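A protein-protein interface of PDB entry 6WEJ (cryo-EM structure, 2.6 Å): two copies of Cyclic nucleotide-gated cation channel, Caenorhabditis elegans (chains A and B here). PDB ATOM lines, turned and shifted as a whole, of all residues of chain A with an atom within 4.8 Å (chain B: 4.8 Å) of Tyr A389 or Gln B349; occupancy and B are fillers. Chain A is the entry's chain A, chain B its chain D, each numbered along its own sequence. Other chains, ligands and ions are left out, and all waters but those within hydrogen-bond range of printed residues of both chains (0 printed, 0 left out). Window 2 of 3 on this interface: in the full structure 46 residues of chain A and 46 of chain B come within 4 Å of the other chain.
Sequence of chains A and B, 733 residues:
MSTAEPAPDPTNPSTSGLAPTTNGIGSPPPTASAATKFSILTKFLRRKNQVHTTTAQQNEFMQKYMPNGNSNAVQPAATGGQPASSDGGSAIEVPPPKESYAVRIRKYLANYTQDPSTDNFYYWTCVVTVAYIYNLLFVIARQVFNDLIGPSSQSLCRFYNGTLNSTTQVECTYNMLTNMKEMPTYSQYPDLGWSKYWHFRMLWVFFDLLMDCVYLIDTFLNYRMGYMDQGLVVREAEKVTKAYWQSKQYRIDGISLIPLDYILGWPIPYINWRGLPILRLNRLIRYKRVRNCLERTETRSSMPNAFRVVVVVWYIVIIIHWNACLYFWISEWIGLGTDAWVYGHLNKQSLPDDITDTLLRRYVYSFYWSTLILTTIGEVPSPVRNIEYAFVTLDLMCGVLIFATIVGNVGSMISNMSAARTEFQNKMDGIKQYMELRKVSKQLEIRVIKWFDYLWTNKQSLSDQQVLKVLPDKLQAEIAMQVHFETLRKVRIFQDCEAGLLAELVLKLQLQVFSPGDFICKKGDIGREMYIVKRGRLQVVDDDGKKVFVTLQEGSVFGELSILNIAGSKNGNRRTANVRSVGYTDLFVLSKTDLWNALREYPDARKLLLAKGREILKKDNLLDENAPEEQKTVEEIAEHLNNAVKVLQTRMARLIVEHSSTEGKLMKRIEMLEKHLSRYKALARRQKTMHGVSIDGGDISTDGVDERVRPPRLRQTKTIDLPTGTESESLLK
The side-chain hydroxyl (OH) of Tyr A389 is in hydrogen-bond range of the backbone carbonyl oxygen (O) of Gln B349 (2.9 Å).
The guanidinium group (NH2) of Arg B361 is in hydrogen-bond range of the backbone carbonyl oxygen (O) of Val A384, 3.4 Å away.
The side-chain amide nitrogen (ND2) of Asn B347 is in hydrogen-bond range of the side-chain hydroxyl (OH) of Tyr B365 (3.0 Å).
The side-chain hydroxyl (OG1) of Thr A393 lies within hydrogen-bond range of the backbone carbonyl oxygen (O) of Tyr A389, 2.6 Å away.
OE1 of Glu A388 sits at hydrogen-bond distance from N of Val A384 (2.8 Å).
NE of Arg B361 sits at hydrogen-bond distance from O of Ser B350 (2.8 Å).
O of Pro A383 lies close to OH of Tyr A389 (3.5 Å).
The side-chain amide oxygen of Asn B347 sits close to the backbone NH of Gln B349 (3.1 Å).
NE2 of Gln B349 touches OG of Ser A382, at 3.7 Å.
Tyr B368 touches Pro A383 (OH to CD, 3.6 Å).
NH1 of Arg B361 touches ND2 of Asn A386, at 3.6 Å.
Arg B361 touches Tyr A389 (NH1 to CE1, 3.4 Å).
Tyr A389 touches Val B364 (CB to CG1, 3.6 Å).
Tyr B365 touches Tyr A389 (CD1 to OH, 3.8 Å).
Tyr B368 touches Tyr A389 (CD2 to CE2, 3.4 Å).
Thr A393 touches Tyr B368 (OG1 to CD1, 3.6 Å).
Tyr A389 touches five residues of chain B.
Gln B349 touches just these residues of chain A: Ser A382 (3.7 Å) and Tyr A389 (2.9 Å).
Printed residues of chain A within 4 Å of Tyr B368: Pro A383, Tyr A389 and Thr A393.
Printed residues of chain B within 4 Å of Val A384: Arg B361 (3.4 Å).
Arg A385 touches none of the printed residues of chain B.
The nearest printed residue of chain B that does not touch Tyr A389 is Ser B350 (4.9 Å).
Hydrophobic or aromatic side chains of chain B within 4 Å of the printed part of chain A: Val B364, Tyr B365 and Tyr B368.
Along chain B the printed residues that touch a printed residue of chain A span positions 349 to 368.
Printed residues of chain A that touch a printed residue of chain B: Ser A382, Pro A383, Val A384, Asn A386, Tyr A389 and Thr A393.
Hydrophobic or aromatic side chains of chain A within 4 Å of the printed part of chain B: Pro A383 and Tyr A389.
Along chain A the printed residues that touch a printed residue of chain B span positions 382 to 393.
No position is printed for both chains.
Of the 10 pairs that touch across the chains among the printed residues, none has its exchanged pair printed and touching as well.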
ATOM      1  N   SER A 382     -25.866 -20.175   1.255  1.00  0.00           N
ATOM      2  CA  SER A 382     -26.708 -21.024   0.435  1.00  0.00           C
ATOM      3  C   SER A 382     -25.870 -21.726  -0.624  1.00  0.00           C
ATOM      4  O   SER A 382     -24.842 -21.202  -1.055  1.00  0.00           O
ATOM      5  CB  SER A 382     -27.794 -20.202  -0.238  1.00  0.00           C
ATOM      6  OG  SER A 382     -28.537 -19.477   0.717  1.00  0.00           O
ATOM      7  N   PRO A 383     -26.287 -22.915  -1.057  1.00  0.00           N
ATOM      8  CA  PRO A 383     -25.564 -23.597  -2.126  1.00  0.00           C
ATOM      9  C   PRO A 383     -25.633 -22.800  -3.413  1.00  0.00           C
ATOM     10  O   PRO A 383     -26.527 -21.982  -3.625  1.00  0.00           O
ATOM     11  CB  PRO A 383     -26.300 -24.928  -2.256  1.00  0.00           C
ATOM     12  CG  PRO A 383     -27.077 -25.066  -1.030  1.00  0.00           C
ATOM     13  CD  PRO A 383     -27.426 -23.709  -0.587  1.00  0.00           C
ATOM     14  N   VAL A 384     -24.660 -23.039  -4.285  1.00  0.00           N
ATOM     15  CA  VAL A 384     -24.559 -22.329  -5.548  1.00  0.00           C
ATOM     16  C   VAL A 384     -24.754 -23.256  -6.736  1.00  0.00           C
ATOM     17  O   VAL A 384     -25.437 -22.899  -7.699  1.00  0.00           O
ATOM     18  CB  VAL A 384     -23.216 -21.585  -5.658  1.00  0.00           C
ATOM     19  CG1 VAL A 384     -23.175 -20.776  -6.917  1.00  0.00           C
ATOM     20  CG2 VAL A 384     -23.013 -20.697  -4.458  1.00  0.00           C
ATOM     21  N   ARG A 385     -24.193 -24.452  -6.682  1.00  0.00           N
ATOM     22  CA  ARG A 385     -24.237 -25.400  -7.780  1.00  0.00           C
ATOM     23  C   ARG A 385     -25.209 -26.530  -7.475  1.00  0.00           C
ATOM     24  O   ARG A 385     -25.616 -26.738  -6.335  1.00  0.00           O
ATOM     25  CB  ARG A 385     -22.843 -25.951  -8.047  1.00  0.00           C
ATOM     26  CG  ARG A 385     -21.855 -24.862  -8.333  1.00  0.00           C
ATOM     27  CD  ARG A 385     -20.453 -25.372  -8.391  1.00  0.00           C
ATOM     28  NE  ARG A 385     -20.273 -26.372  -9.427  1.00  0.00           N
ATOM     29  CZ  ARG A 385     -19.093 -26.696  -9.936  1.00  0.00           C
ATOM     30  NH1 ARG A 385     -18.000 -26.088  -9.509  1.00  0.00           N
ATOM     31  NH2 ARG A 385     -19.007 -27.621 -10.876  1.00  0.00           N
ATOM     32  N   ASN A 386     -25.580 -27.259  -8.524  1.00  0.00           N
ATOM     33  CA  ASN A 386     -26.566 -28.325  -8.383  1.00  0.00           C
ATOM     34  C   ASN A 386     -26.071 -29.417  -7.448  1.00  0.00           C
ATOM     35  O   ASN A 386     -26.853 -29.992  -6.684  1.00  0.00           O
ATOM     36  CB  ASN A 386     -26.895 -28.911  -9.754  1.00  0.00           C
ATOM     37  CG  ASN A 386     -27.690 -27.965 -10.620  1.00  0.00           C
ATOM     38  OD1 ASN A 386     -28.811 -28.260 -10.995  1.00  0.00           O
ATOM     39  ND2 ASN A 386     -27.115 -26.825 -10.944  1.00  0.00           N
ATOM     40  N   ILE A 387     -24.772 -29.710  -7.485  1.00  0.00           N
ATOM     41  CA  ILE A 387     -24.224 -30.753  -6.630  1.00  0.00           C
ATOM     42  C   ILE A 387     -24.222 -30.300  -5.173  1.00  0.00           C
ATOM     43  O   ILE A 387     -24.498 -31.089  -4.262  1.00  0.00           O
ATOM     44  CB  ILE A 387     -22.823 -31.156  -7.128  1.00  0.00           C
ATOM     45  CG1 ILE A 387     -22.339 -32.415  -6.418  1.00  0.00           C
ATOM     46  CG2 ILE A 387     -21.830 -30.025  -6.985  1.00  0.00           C
ATOM     47  CD1 ILE A 387     -23.133 -33.637  -6.776  1.00  0.00           C
ATOM     48  N   GLU A 388     -23.955 -29.015  -4.934  1.00  0.00           N
ATOM     49  CA  GLU A 388     -24.037 -28.477  -3.584  1.00  0.00           C
ATOM     50  C   GLU A 388     -25.472 -28.463  -3.089  1.00  0.00           C
ATOM     51  O   GLU A 388     -25.725 -28.705  -1.908  1.00  0.00           O
ATOM     52  CB  GLU A 388     -23.454 -27.074  -3.545  1.00  0.00           C
ATOM     53  CG  GLU A 388     -22.058 -26.978  -4.071  1.00  0.00           C
ATOM     54  CD  GLU A 388     -21.610 -25.556  -4.196  1.00  0.00           C
ATOM     55  OE1 GLU A 388     -22.414 -24.667  -3.895  1.00  0.00           O
ATOM     56  OE2 GLU A 388     -20.462 -25.318  -4.595  1.00  0.00           O
ATOM     57  N   TYR A 389     -26.426 -28.190  -3.980  1.00  0.00           N
ATOM     58  CA  TYR A 389     -27.832 -28.255  -3.603  1.00  0.00           C
ATOM     59  C   TYR A 389     -28.230 -29.663  -3.206  1.00  0.00           C
ATOM     60  O   TYR A 389     -28.934 -29.854  -2.212  1.00  0.00           O
ATOM     61  CB  TYR A 389     -28.706 -27.767  -4.752  1.00  0.00           C
ATOM     62  CG  TYR A 389     -29.006 -26.298  -4.716  1.00  0.00           C
ATOM     63  CD1 TYR A 389     -28.155 -25.388  -5.290  1.00  0.00           C
ATOM     64  CD2 TYR A 389     -30.144 -25.823  -4.110  1.00  0.00           C
ATOM     65  CE1 TYR A 389     -28.426 -24.051  -5.255  1.00  0.00           C
ATOM     66  CE2 TYR A 389     -30.419 -24.490  -4.074  1.00  0.00           C
ATOM     67  CZ  TYR A 389     -29.558 -23.608  -4.643  1.00  0.00           C
ATOM     68  OH  TYR A 389     -29.830 -22.268  -4.605  1.00  0.00           O
ATOM     69  N   ALA A 390     -27.790 -30.665  -3.966  1.00  0.00           N
ATOM     70  CA  ALA A 390     -28.103 -32.046  -3.619  1.00  0.00           C
ATOM     71  C   ALA A 390     -27.502 -32.426  -2.274  1.00  0.00           C
ATOM     72  O   ALA A 390     -28.180 -33.005  -1.414  1.00  0.00           O
ATOM     73  CB  ALA A 390     -27.602 -32.979  -4.716  1.00  0.00           C
ATOM     74  N   PHE A 391     -26.222 -32.097  -2.074  1.00  0.00           N
ATOM     75  CA  PHE A 391     -25.564 -32.399  -0.809  1.00  0.00           C
ATOM     76  C   PHE A 391     -26.276 -31.732   0.359  1.00  0.00           C
ATOM     77  O   PHE A 391     -26.547 -32.375   1.374  1.00  0.00           O
ATOM     78  CB  PHE A 391     -24.101 -31.970  -0.865  1.00  0.00           C
ATOM     79  CG  PHE A 391     -23.396 -32.030   0.458  1.00  0.00           C
ATOM     80  CD1 PHE A 391     -23.300 -33.216   1.156  1.00  0.00           C
ATOM     81  CD2 PHE A 391     -22.822 -30.903   1.003  1.00  0.00           C
ATOM     82  CE1 PHE A 391     -22.653 -33.263   2.366  1.00  0.00           C
ATOM     83  CE2 PHE A 391     -22.178 -30.956   2.213  1.00  0.00           C
ATOM     84  CZ  PHE A 391     -22.094 -32.134   2.891  1.00  0.00           C
ATOM     85  N   VAL A 392     -26.600 -30.446   0.229  1.00  0.00           N
ATOM     86  CA  VAL A 392     -27.178 -29.715   1.348  1.00  0.00           C
ATOM     87  C   VAL A 392     -28.609 -30.160   1.609  1.00  0.00           C
ATOM     88  O   VAL A 392     -29.052 -30.191   2.756  1.00  0.00           O
ATOM     89  CB  VAL A 392     -27.082 -28.204   1.097  1.00  0.00           C
ATOM     90  CG1 VAL A 392     -27.831 -27.446   2.154  1.00  0.00           C
ATOM     91  CG2 VAL A 392     -25.644 -27.781   1.097  1.00  0.00           C
ATOM     92  N   THR A 393     -29.356 -30.524   0.568  1.00  0.00           N
ATOM     93  CA  THR A 393     -30.709 -31.025   0.779  1.00  0.00           C
ATOM     94  C   THR A 393     -30.683 -32.341   1.541  1.00  0.00           C
ATOM     95  O   THR A 393     -31.415 -32.522   2.524  1.00  0.00           O
ATOM     96  CB  THR A 393     -31.412 -31.192  -0.565  1.00  0.00           C
ATOM     97  OG1 THR A 393     -31.347 -29.964  -1.288  1.00  0.00           O
ATOM     98  CG2 THR A 393     -32.854 -31.553  -0.364  1.00  0.00           C
ATOM     99  N   ASN B 347     -34.595 -13.613  -8.580  1.00  0.00           N
ATOM    100  CA  ASN B 347     -34.290 -14.449  -7.427  1.00  0.00           C
ATOM    101  C   ASN B 347     -32.846 -14.893  -7.591  1.00  0.00           C
ATOM    102  O   ASN B 347     -32.545 -15.798  -8.365  1.00  0.00           O
ATOM    103  CB  ASN B 347     -35.253 -15.628  -7.355  1.00  0.00           C
ATOM    104  CG  ASN B 347     -35.092 -16.443  -6.104  1.00  0.00           C
ATOM    105  OD1 ASN B 347     -34.125 -16.294  -5.379  1.00  0.00           O
ATOM    106  ND2 ASN B 347     -36.037 -17.323  -5.850  1.00  0.00           N
ATOM    107  N   LYS B 348     -31.939 -14.233  -6.881  1.00  0.00           N
ATOM    108  CA  LYS B 348     -30.514 -14.497  -7.012  1.00  0.00           C
ATOM    109  C   LYS B 348     -30.072 -15.747  -6.276  1.00  0.00           C
ATOM    110  O   LYS B 348     -28.880 -16.051  -6.266  1.00  0.00           O
ATOM    111  CB  LYS B 348     -29.712 -13.299  -6.515  1.00  0.00           C
ATOM    112  CG  LYS B 348     -29.128 -12.461  -7.618  1.00  0.00           C
ATOM    113  CD  LYS B 348     -30.200 -11.901  -8.509  1.00  0.00           C
ATOM    114  CE  LYS B 348     -29.604 -11.190  -9.702  1.00  0.00           C
ATOM    115  NZ  LYS B 348     -30.656 -10.661 -10.610  1.00  0.00           N
ATOM    116  N   GLN B 349     -30.993 -16.463  -5.649  1.00  0.00           N
ATOM    117  CA  GLN B 349     -30.697 -17.786  -5.129  1.00  0.00           C
ATOM    118  C   GLN B 349     -31.093 -18.873  -6.112  1.00  0.00           C
ATOM    119  O   GLN B 349     -30.460 -19.932  -6.141  1.00  0.00           O
ATOM    120  CB  GLN B 349     -31.406 -17.991  -3.793  1.00  0.00           C
ATOM    121  CG  GLN B 349     -31.058 -19.281  -3.102  1.00  0.00           C
ATOM    122  CD  GLN B 349     -31.687 -19.393  -1.742  1.00  0.00           C
ATOM    123  OE1 GLN B 349     -32.277 -18.447  -1.249  1.00  0.00           O
ATOM    124  NE2 GLN B 349     -31.561 -20.549  -1.126  1.00  0.00           N
ATOM    125  N   SER B 350     -32.124 -18.631  -6.923  1.00  0.00           N
ATOM    126  CA  SER B 350     -32.438 -19.517  -8.035  1.00  0.00           C
ATOM    127  C   SER B 350     -31.288 -19.560  -9.018  1.00  0.00           C
ATOM    128  O   SER B 350     -30.738 -20.622  -9.315  1.00  0.00           O
ATOM    129  CB  SER B 350     -33.700 -19.045  -8.747  1.00  0.00           C
ATOM    130  OG  SER B 350     -34.796 -19.018  -7.875  1.00  0.00           O
ATOM    131  N   LEU B 351     -30.914 -18.395  -9.536  1.00  0.00           N
ATOM    132  CA  LEU B 351     -29.923 -18.267 -10.593  1.00  0.00           C
ATOM    133  C   LEU B 351     -28.809 -17.357 -10.103  1.00  0.00           C
ATOM    134  O   LEU B 351     -28.845 -16.140 -10.327  1.00  0.00           O
ATOM    135  CB  LEU B 351     -30.569 -17.739 -11.870  1.00  0.00           C
ATOM    136  CG  LEU B 351     -31.634 -18.683 -12.419  1.00  0.00           C
ATOM    137  CD1 LEU B 351     -32.387 -18.057 -13.550  1.00  0.00           C
ATOM    138  CD2 LEU B 351     -30.977 -19.959 -12.857  1.00  0.00           C
ATOM    139  N   PRO B 352     -27.809 -17.904  -9.433  1.00  0.00           N
ATOM    140  CA  PRO B 352     -26.619 -17.123  -9.094  1.00  0.00           C
ATOM    141  C   PRO B 352     -25.786 -16.817 -10.323  1.00  0.00           C
ATOM    142  O   PRO B 352     -26.244 -17.006 -11.452  1.00  0.00           O
ATOM    143  CB  PRO B 352     -25.873 -18.034  -8.118  1.00  0.00           C
ATOM    144  CG  PRO B 352     -26.891 -18.938  -7.590  1.00  0.00           C
ATOM    145  CD  PRO B 352     -27.837 -19.176  -8.703  1.00  0.00           C
ATOM    146  N   ARG B 361     -32.095 -27.435 -13.085  1.00  0.00           N
ATOM    147  CA  ARG B 361     -31.991 -26.346 -12.124  1.00  0.00           C
ATOM    148  C   ARG B 361     -33.350 -25.978 -11.556  1.00  0.00           C
ATOM    149  O   ARG B 361     -33.475 -25.727 -10.355  1.00  0.00           O
ATOM    150  CB  ARG B 361     -31.338 -25.135 -12.776  1.00  0.00           C
ATOM    151  CG  ARG B 361     -31.137 -23.964 -11.849  1.00  0.00           C
ATOM    152  CD  ARG B 361     -30.324 -24.373 -10.657  1.00  0.00           C
ATOM    153  NE  ARG B 361     -29.933 -23.242  -9.832  1.00  0.00           N
ATOM    154  CZ  ARG B 361     -29.044 -23.322  -8.854  1.00  0.00           C
ATOM    155  NH1 ARG B 361     -28.464 -24.473  -8.591  1.00  0.00           N
ATOM    156  NH2 ARG B 361     -28.735 -22.254  -8.146  1.00  0.00           N
ATOM    157  N   VAL B 364     -34.342 -28.733  -9.117  1.00  0.00           N
ATOM    158  CA  VAL B 364     -33.455 -28.795  -7.964  1.00  0.00           C
ATOM    159  C   VAL B 364     -33.723 -27.632  -7.021  1.00  0.00           C
ATOM    160  O   VAL B 364     -33.838 -27.814  -5.803  1.00  0.00           O
ATOM    161  CB  VAL B 364     -31.991 -28.833  -8.432  1.00  0.00           C
ATOM    162  CG1 VAL B 364     -31.064 -28.385  -7.341  1.00  0.00           C
ATOM    163  CG2 VAL B 364     -31.633 -30.224  -8.878  1.00  0.00           C
ATOM    164  N   TYR B 365     -33.849 -26.423  -7.563  1.00  0.00           N
ATOM    165  CA  TYR B 365     -34.132 -25.284  -6.706  1.00  0.00           C
ATOM    166  C   TYR B 365     -35.518 -25.378  -6.094  1.00  0.00           C
ATOM    167  O   TYR B 365     -35.708 -24.994  -4.939  1.00  0.00           O
ATOM    168  CB  TYR B 365     -33.987 -23.976  -7.469  1.00  0.00           C
ATOM    169  CG  TYR B 365     -34.355 -22.808  -6.597  1.00  0.00           C
ATOM    170  CD1 TYR B 365     -33.484 -22.353  -5.625  1.00  0.00           C
ATOM    171  CD2 TYR B 365     -35.586 -22.185  -6.717  1.00  0.00           C
ATOM    172  CE1 TYR B 365     -33.818 -21.311  -4.815  1.00  0.00           C
ATOM    173  CE2 TYR B 365     -35.924 -21.138  -5.907  1.00  0.00           C
ATOM    174  CZ  TYR B 365     -35.034 -20.707  -4.959  1.00  0.00           C
ATOM    175  OH  TYR B 365     -35.357 -19.658  -4.144  1.00  0.00           O
ATOM    176  N   TYR B 368     -35.323 -27.798  -3.217  1.00  0.00           N
ATOM    177  CA  TYR B 368     -34.630 -27.198  -2.084  1.00  0.00           C
ATOM    178  C   TYR B 368     -35.519 -26.195  -1.357  1.00  0.00           C
ATOM    179  O   TYR B 368     -35.588 -26.192  -0.124  1.00  0.00           O
ATOM    180  CB  TYR B 368     -33.345 -26.539  -2.569  1.00  0.00           C
ATOM    181  CG  TYR B 368     -32.575 -25.797  -1.511  1.00  0.00           C
ATOM    182  CD1 TYR B 368     -31.776 -26.473  -0.608  1.00  0.00           C
ATOM    183  CD2 TYR B 368     -32.628 -24.417  -1.430  1.00  0.00           C
ATOM    184  CE1 TYR B 368     -31.069 -25.800   0.342  1.00  0.00           C
ATOM    185  CE2 TYR B 368     -31.922 -23.739  -0.483  1.00  0.00           C
ATOM    186  CZ  TYR B 368     -31.145 -24.433   0.400  1.00  0.00           C
ATOM    187  OH  TYR B 368     -30.437 -23.749   1.352  1.00  0.00           O
ATOM    188  N   GLU B 379     -34.823 -20.637   5.134  1.00  0.00           N
ATOM    189  CA  GLU B 379     -33.723 -19.821   4.640  1.00  0.00           C
ATOM    190  C   GLU B 379     -33.889 -19.544   3.154  1.00  0.00           C
ATOM    191  O   GLU B 379     -32.970 -19.775   2.365  1.00  0.00           O
ATOM    192  CB  GLU B 379     -32.391 -20.509   4.910  1.00  0.00           C
ATOM    193  CG  GLU B 379     -32.112 -20.741   6.372  1.00  0.00           C
ATOM    194  CD  GLU B 379     -31.808 -19.463   7.107  1.00  0.00           C
ATOM    195  OE1 GLU B 379     -31.241 -18.543   6.490  1.00  0.00           O
ATOM    196  OE2 GLU B 379     -32.140 -19.375   8.304  1.00  0.00           O
ATOM    197  N   VAL B 380     -35.055 -19.041   2.771  1.00  0.00           N
ATOM    198  CA  VAL B 380     -35.390 -18.790   1.373  1.00  0.00           C
ATOM    199  C   VAL B 380     -35.831 -17.338   1.258  1.00  0.00           C
ATOM    200  O   VAL B 380     -36.167 -16.703   2.267  1.00  0.00           O
ATOM    201  CB  VAL B 380     -36.488 -19.757   0.870  1.00  0.00           C
ATOM    202  CG1 VAL B 380     -35.937 -21.155   0.731  1.00  0.00           C
ATOM    203  CG2 VAL B 380     -37.652 -19.767   1.817  1.00  0.00           C
ATOM    204  N   PRO B 381     -35.816 -16.776   0.049  1.00  0.00           N
ATOM    205  CA  PRO B 381     -36.265 -15.392  -0.118  1.00  0.00           C
ATOM    206  C   PRO B 381     -37.661 -15.163   0.444  1.00  0.00           C
ATOM    207  O   PRO B 381     -38.493 -16.068   0.491  1.00  0.00           O
ATOM    208  CB  PRO B 381     -36.232 -15.201  -1.636  1.00  0.00           C
ATOM    209  CG  PRO B 381     -35.165 -16.084  -2.069  1.00  0.00           C
ATOM    210  CD  PRO B 381     -35.237 -17.296  -1.196  1.00  0.00           C
